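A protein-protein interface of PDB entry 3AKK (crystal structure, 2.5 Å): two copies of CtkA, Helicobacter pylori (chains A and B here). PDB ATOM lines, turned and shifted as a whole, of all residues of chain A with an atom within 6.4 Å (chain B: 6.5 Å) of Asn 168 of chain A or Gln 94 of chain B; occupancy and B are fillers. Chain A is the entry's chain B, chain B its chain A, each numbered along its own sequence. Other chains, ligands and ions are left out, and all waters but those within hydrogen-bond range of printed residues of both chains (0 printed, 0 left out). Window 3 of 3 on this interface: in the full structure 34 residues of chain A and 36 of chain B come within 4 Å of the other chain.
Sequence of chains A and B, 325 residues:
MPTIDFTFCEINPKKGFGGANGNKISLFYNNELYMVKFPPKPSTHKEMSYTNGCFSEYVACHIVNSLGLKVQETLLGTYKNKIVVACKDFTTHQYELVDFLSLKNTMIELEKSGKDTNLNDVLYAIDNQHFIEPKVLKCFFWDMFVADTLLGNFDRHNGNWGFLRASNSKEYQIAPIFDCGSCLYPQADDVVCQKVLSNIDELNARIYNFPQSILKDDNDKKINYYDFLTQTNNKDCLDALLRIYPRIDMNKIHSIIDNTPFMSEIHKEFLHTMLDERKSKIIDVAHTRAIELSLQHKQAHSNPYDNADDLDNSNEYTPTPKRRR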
ATOM      1  N   GLN A  94     -23.141  -6.446 -11.500  1.00  0.00           N
ATOM      2  CA  GLN A  94     -24.336  -7.228 -11.779  1.00  0.00           C
ATOM      3  C   GLN A  94     -24.708  -7.214 -13.247  1.00  0.00           C
ATOM      4  O   GLN A  94     -25.784  -7.679 -13.617  1.00  0.00           O
ATOM      5  CB  GLN A  94     -25.530  -6.722 -10.954  1.00  0.00           C
ATOM      6  CG  GLN A  94     -26.150  -7.746 -10.008  1.00  0.00           C
ATOM      7  CD  GLN A  94     -25.467  -7.779  -8.657  1.00  0.00           C
ATOM      8  OE1 GLN A  94     -25.902  -7.117  -7.715  1.00  0.00           O
ATOM      9  NE2 GLN A  94     -24.383  -8.542  -8.557  1.00  0.00           N
ATOM     10  N   GLU A  96     -24.490  -8.558 -17.051  1.00  0.00           N
ATOM     11  CA  GLU A  96     -24.232  -9.866 -17.647  1.00  0.00           C
ATOM     12  C   GLU A  96     -24.323  -9.775 -19.159  1.00  0.00           C
ATOM     13  O   GLU A  96     -25.213  -9.121 -19.698  1.00  0.00           O
ATOM     14  CB  GLU A  96     -25.204 -10.916 -17.109  1.00  0.00           C
ATOM     15  CG  GLU A  96     -25.042 -11.204 -15.621  1.00  0.00           C
ATOM     16  CD  GLU A  96     -25.024 -12.697 -15.302  1.00  0.00           C
ATOM     17  OE1 GLU A  96     -24.732 -13.510 -16.216  1.00  0.00           O
ATOM     18  OE2 GLU A  96     -25.295 -13.053 -14.131  1.00  0.00           O
ATOM     19  N   ARG A 165     -27.466  -7.430 -19.750  1.00  0.00           N
ATOM     20  CA  ARG A 165     -28.649  -7.375 -18.906  1.00  0.00           C
ATOM     21  C   ARG A 165     -28.221  -7.167 -17.475  1.00  0.00           C
ATOM     22  O   ARG A 165     -27.394  -7.909 -16.945  1.00  0.00           O
ATOM     23  CB  ARG A 165     -29.514  -8.635 -19.037  1.00  0.00           C
ATOM     24  CG  ARG A 165     -28.819  -9.946 -18.691  1.00  0.00           C
ATOM     25  CD  ARG A 165     -29.836 -10.980 -18.180  1.00  0.00           C
ATOM     26  NE  ARG A 165     -31.201 -10.650 -18.594  1.00  0.00           N
ATOM     27  CZ  ARG A 165     -32.187 -10.309 -17.764  1.00  0.00           C
ATOM     28  NH1 ARG A 165     -31.978 -10.267 -16.449  1.00  0.00           N
ATOM     29  NH2 ARG A 165     -33.388 -10.024 -18.251  1.00  0.00           N
ATOM     30  N   ALA A 166     -28.763  -6.131 -16.856  1.00  0.00           N
ATOM     31  CA  ALA A 166     -28.549  -5.935 -15.434  1.00  0.00           C
ATOM     32  C   ALA A 166     -29.243  -7.092 -14.760  1.00  0.00           C
ATOM     33  O   ALA A 166     -30.317  -7.508 -15.193  1.00  0.00           O
ATOM     34  CB  ALA A 166     -29.143  -4.623 -14.982  1.00  0.00           C
ATOM     35  N   SER A 167     -28.625  -7.641 -13.725  1.00  0.00           N
ATOM     36  CA  SER A 167     -29.260  -8.719 -12.977  1.00  0.00           C
ATOM     37  C   SER A 167     -30.542  -8.198 -12.342  1.00  0.00           C
ATOM     38  O   SER A 167     -30.668  -6.999 -12.084  1.00  0.00           O
ATOM     39  CB  SER A 167     -28.324  -9.244 -11.890  1.00  0.00           C
ATOM     40  OG  SER A 167     -28.959  -9.202 -10.618  1.00  0.00           O
ATOM     41  N   ASN A 168     -31.489  -9.098 -12.107  1.00  0.00           N
ATOM     42  CA  ASN A 168     -32.747  -8.779 -11.419  1.00  0.00           C
ATOM     43  C   ASN A 168     -33.768  -7.971 -12.227  1.00  0.00           C
ATOM     44  O   ASN A 168     -34.868  -7.686 -11.743  1.00  0.00           O
ATOM     45  CB  ASN A 168     -32.504  -8.168 -10.025  1.00  0.00           C
ATOM     46  CG  ASN A 168     -32.247  -6.663 -10.054  1.00  0.00           C
ATOM     47  OD1 ASN A 168     -32.505  -5.969 -11.051  1.00  0.00           O
ATOM     48  ND2 ASN A 168     -31.744  -6.146  -8.933  1.00  0.00           N
ATOM     49  N   SER A 169     -33.406  -7.621 -13.457  1.00  0.00           N
ATOM     50  CA  SER A 169     -34.308  -6.890 -14.346  1.00  0.00           C
ATOM     51  C   SER A 169     -34.537  -7.674 -15.634  1.00  0.00           C
ATOM     52  O   SER A 169     -33.868  -8.677 -15.897  1.00  0.00           O
ATOM     53  CB  SER A 169     -33.755  -5.492 -14.656  1.00  0.00           C
ATOM     54  OG  SER A 169     -34.637  -4.773 -15.503  1.00  0.00           O
ATOM     55  N   LYS A 170     -35.498  -7.214 -16.424  1.00  0.00           N
ATOM     56  CA  LYS A 170     -35.766  -7.776 -17.745  1.00  0.00           C
ATOM     57  C   LYS A 170     -35.138  -6.889 -18.830  1.00  0.00           C
ATOM     58  O   LYS A 170     -35.380  -7.080 -20.029  1.00  0.00           O
ATOM     59  CB  LYS A 170     -37.283  -7.911 -17.949  1.00  0.00           C
ATOM     60  CG  LYS A 170     -37.730  -8.149 -19.387  1.00  0.00           C
ATOM     61  CD  LYS A 170     -39.247  -8.205 -19.513  1.00  0.00           C
ATOM     62  CE  LYS A 170     -39.823  -9.411 -18.785  1.00  0.00           C
ATOM     63  NZ  LYS A 170     -41.307  -9.433 -18.881  1.00  0.00           N
ATOM     64  N   THR B  91     -30.059 -21.589 -14.618  1.00  0.00           N
ATOM     65  CA  THR B  91     -29.498 -20.238 -14.490  1.00  0.00           C
ATOM     66  C   THR B  91     -30.614 -19.228 -14.224  1.00  0.00           C
ATOM     67  O   THR B  91     -30.608 -18.106 -14.705  1.00  0.00           O
ATOM     68  CB  THR B  91     -28.752 -19.827 -15.746  1.00  0.00           C
ATOM     69  OG1 THR B  91     -29.566 -20.132 -16.883  1.00  0.00           O
ATOM     70  CG2 THR B  91     -27.441 -20.572 -15.840  1.00  0.00           C
ATOM     71  N   THR B  92     -31.579 -19.672 -13.449  1.00  0.00           N
ATOM     72  CA  THR B  92     -32.750 -18.898 -13.114  1.00  0.00           C
ATOM     73  C   THR B  92     -32.571 -18.467 -11.650  1.00  0.00           C
ATOM     74  O   THR B  92     -31.655 -18.950 -10.971  1.00  0.00           O
ATOM     75  CB  THR B  92     -33.979 -19.800 -13.316  1.00  0.00           C
ATOM     76  OG1 THR B  92     -34.768 -19.312 -14.407  1.00  0.00           O
ATOM     77  CG2 THR B  92     -34.801 -19.908 -12.070  1.00  0.00           C
ATOM     78  N   HIS B  93     -33.414 -17.562 -11.155  1.00  0.00           N
ATOM     79  CA  HIS B  93     -33.252 -17.075  -9.779  1.00  0.00           C
ATOM     80  C   HIS B  93     -31.867 -16.463  -9.599  1.00  0.00           C
ATOM     81  O   HIS B  93     -31.251 -16.582  -8.536  1.00  0.00           O
ATOM     82  CB  HIS B  93     -33.489 -18.196  -8.753  1.00  0.00           C
ATOM     83  CG  HIS B  93     -34.917 -18.641  -8.673  1.00  0.00           C
ATOM     84  ND1 HIS B  93     -35.758 -18.269  -7.645  1.00  0.00           N
ATOM     85  CD2 HIS B  93     -35.663 -19.398  -9.512  1.00  0.00           C
ATOM     86  CE1 HIS B  93     -36.955 -18.792  -7.846  1.00  0.00           C
ATOM     87  NE2 HIS B  93     -36.924 -19.482  -8.975  1.00  0.00           N
ATOM     88  N   GLN B  94     -31.381 -15.822 -10.662  1.00  0.00           N
ATOM     89  CA  GLN B  94     -30.179 -14.996 -10.604  1.00  0.00           C
ATOM     90  C   GLN B  94     -28.910 -15.815 -10.422  1.00  0.00           C
ATOM     91  O   GLN B  94     -28.107 -15.531  -9.540  1.00  0.00           O
ATOM     92  CB  GLN B  94     -30.286 -13.946  -9.483  1.00  0.00           C
ATOM     93  CG  GLN B  94     -31.496 -13.021  -9.582  1.00  0.00           C
ATOM     94  CD  GLN B  94     -31.605 -12.328 -10.933  1.00  0.00           C
ATOM     95  OE1 GLN B  94     -30.640 -11.738 -11.424  1.00  0.00           O
ATOM     96  NE2 GLN B  94     -32.790 -12.390 -11.538  1.00  0.00           N
ATOM     97  N   TYR B  95     -28.735 -16.838 -11.246  1.00  0.00           N
ATOM     98  CA  TYR B  95     -27.458 -17.528 -11.302  1.00  0.00           C
ATOM     99  C   TYR B  95     -26.903 -17.390 -12.695  1.00  0.00           C
ATOM    100  O   TYR B  95     -27.633 -17.513 -13.666  1.00  0.00           O
ATOM    101  CB  TYR B  95     -27.601 -19.013 -10.967  1.00  0.00           C
ATOM    102  CG  TYR B  95     -27.765 -19.315  -9.497  1.00  0.00           C
ATOM    103  CD1 TYR B  95     -29.002 -19.700  -8.988  1.00  0.00           C
ATOM    104  CD2 TYR B  95     -26.693 -19.228  -8.625  1.00  0.00           C
ATOM    105  CE1 TYR B  95     -29.173 -19.984  -7.654  1.00  0.00           C
ATOM    106  CE2 TYR B  95     -26.849 -19.508  -7.287  1.00  0.00           C
ATOM    107  CZ  TYR B  95     -28.099 -19.889  -6.804  1.00  0.00           C
ATOM    108  OH  TYR B  95     -28.290 -20.176  -5.468  1.00  0.00           O
ATOM    109  N   GLU B  96     -25.612 -17.127 -12.806  1.00  0.00           N
ATOM    110  CA  GLU B  96     -24.977 -17.200 -14.111  1.00  0.00           C
ATOM    111  C   GLU B  96     -24.186 -18.491 -14.226  1.00  0.00           C
ATOM    112  O   GLU B  96     -23.543 -18.936 -13.273  1.00  0.00           O
ATOM    113  CB  GLU B  96     -24.076 -15.997 -14.371  1.00  0.00           C
ATOM    114  CG  GLU B  96     -22.783 -16.372 -15.095  1.00  0.00           C
ATOM    115  CD  GLU B  96     -22.062 -15.187 -15.725  1.00  0.00           C
ATOM    116  OE1 GLU B  96     -22.152 -15.046 -16.968  1.00  0.00           O
ATOM    117  OE2 GLU B  96     -21.399 -14.413 -14.985  1.00  0.00           O
ATOM    118  N   ARG B 165     -22.719 -19.098 -10.367  1.00  0.00           N
ATOM    119  CA  ARG B 165     -22.384 -17.935  -9.585  1.00  0.00           C
ATOM    120  C   ARG B 165     -23.650 -17.186  -9.259  1.00  0.00           C
ATOM    121  O   ARG B 165     -24.461 -16.973 -10.086  1.00  0.00           O
ATOM    122  CB  ARG B 165     -21.453 -17.020 -10.369  1.00  0.00           C
ATOM    123  CG  ARG B 165     -20.840 -15.917  -9.524  1.00  0.00           C
ATOM    124  CD  ARG B 165     -20.374 -14.700 -10.291  1.00  0.00           C
ATOM    125  NE  ARG B 165     -21.019 -14.422 -11.555  1.00  0.00           N
ATOM    126  CZ  ARG B 165     -21.712 -13.322 -11.814  1.00  0.00           C
ATOM    127  NH1 ARG B 165     -22.235 -13.108 -12.982  1.00  0.00           N
ATOM    128  NH2 ARG B 165     -21.868 -12.431 -10.890  1.00  0.00           N
ATOM    129  N   ALA B 166     -23.800 -16.768  -8.023  1.00  0.00           N
ATOM    130  CA  ALA B 166     -24.961 -15.986  -7.678  1.00  0.00           C
ATOM    131  C   ALA B 166     -24.698 -14.590  -8.143  1.00  0.00           C
ATOM    132  O   ALA B 166     -23.778 -13.978  -7.675  1.00  0.00           O
ATOM    133  CB  ALA B 166     -25.196 -16.009  -6.243  1.00  0.00           C
ATOM    134  N   SER B 167     -25.489 -14.114  -9.089  1.00  0.00           N
ATOM    135  CA  SER B 167     -25.435 -12.744  -9.539  1.00  0.00           C
ATOM    136  C   SER B 167     -25.227 -11.763  -8.404  1.00  0.00           C
ATOM    137  O   SER B 167     -24.411 -10.858  -8.510  1.00  0.00           O
ATOM    138  CB  SER B 167     -26.698 -12.371 -10.300  1.00  0.00           C
ATOM    139  OG  SER B 167     -26.448 -11.304 -11.186  1.00  0.00           O
ATOM    140  N   ASN B 168     -25.966 -11.915  -7.322  1.00  0.00           N
ATOM    141  CA  ASN B 168     -25.603 -11.157  -6.167  1.00  0.00           C
ATOM    142  C   ASN B 168     -24.096 -11.183  -6.255  1.00  0.00           C
ATOM    143  O   ASN B 168     -23.461 -10.205  -6.521  1.00  0.00           O
ATOM    144  CB  ASN B 168     -26.121 -11.802  -4.902  1.00  0.00           C
ATOM    145  CG  ASN B 168     -26.515 -10.777  -3.840  1.00  0.00           C
ATOM    146  OD1 ASN B 168     -25.782  -9.835  -3.592  1.00  0.00           O
ATOM    147  ND2 ASN B 168     -27.665 -10.974  -3.205  1.00  0.00           N
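Printed residues of chain B that touch a printed residue of chain A: Gln 94, Glu 96, Arg 165, Ser 167 and Asn 168. Along chain B the printed residues that touch a printed residue of chain A span positions 94 to 168. Of the 8 printed residues of chain A, 4 touch a printed residue of chain B. Printed residues of chain A that touch a printed residue of chain B: Gln 94, Glu 96, Ser 167 and Asn 168. Among the printed residues, 8 pairs touch across the chains. Among the printed residues, Asp or Glu carboxylates within 4 Å of a Lys or Arg side-chain nitrogen of the other chain: Glu 96 of chain A with Arg 165 of chain B.
Gln 94 of chain A touches Asn 168 of chain B, and with the chains exchanged Asn 168 of chain A touches Gln 94 of chain B. Glu 96 of chain A touches its own counterpart, Glu 96 of chain B. Glu 96 of chain A touches Ser 167 of chain B, but with the chains exchanged Ser 167 of chain A does not touch Glu 96 of chain B (8.4 Å). Ser 167 of chain A touches its own counterpart, Ser 167 of chain B.
The backbone carbonyl oxygen (O) of Gln 94 of chain B sits at hydrogen-bond distance from the backbone NH (N) of Ser 167 of chain B, at 3.0 Å. OE2 of Glu 96 of chain B lies within salt-bridge range of NH1 of Arg 165 of chain B. The backbone carbonyl oxygen of Gln 94 of chain A lies within hydrogen-bond range of the backbone NH of Ser 167 of chain A. O of Glu 96 of chain A is in hydrogen-bond range of N of Arg 165 of chain A (2.8 Å).
OG of Ser 167 of chain A lies within hydrogen-bond range of OE1 of Gln 94 of chain B, at 3.1 Å. N of Asn 168 of chain A sits at hydrogen-bond distance from OE1 of Gln 94 of chain B. The side-chain carboxylate (OE2) of Glu 96 of chain A lies within salt-bridge range of the guanidinium group (NH1) of Arg 165 of chain B (3.3 Å). The side-chain hydroxyl (OG) of Ser 167 of chain B lies close to the side-chain hydroxyl (OG) of Ser 167 of chain A (3.3 Å). O of Asn 168 of chain B lies within hydrogen-bond range of NE2 of Gln 94 of chain A (2.8 Å). The side-chain amide nitrogen of Gln 94 of chain A lies close to the backbone carbonyl oxygen of Ser 167 of chain B, 2.3 Å away. The side-chain carboxylate of Glu 96 of chain A sits close to the side-chain carboxylate of Glu 96 of chain B, at 3.1 Å.
Printed residues of chain B within 4 Å of Gln 94 of chain A: Ser 167 and Asn 168. Printed residues of chain B within 4 Å of Glu 96 of chain A: Glu 96 (3.1 Å), Arg 165 (3.3 Å) and Ser 167 (3.6 Å). Of the printed residues of chain B, Ser 167 of chain A touches Gln 94 and Ser 167. Of the printed residues of chain A, Gln 94 of chain B touches Ser 167 (3.1 Å) and Asn 168 (2.9 Å). The nearest residue of chain A that does not touch Gln 94 of chain B is Ser 169 of chain A (5.2 Å).
OG of Ser 167 of chain B touches OE2 of Glu 96 of chain A, at 3.6 Å.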
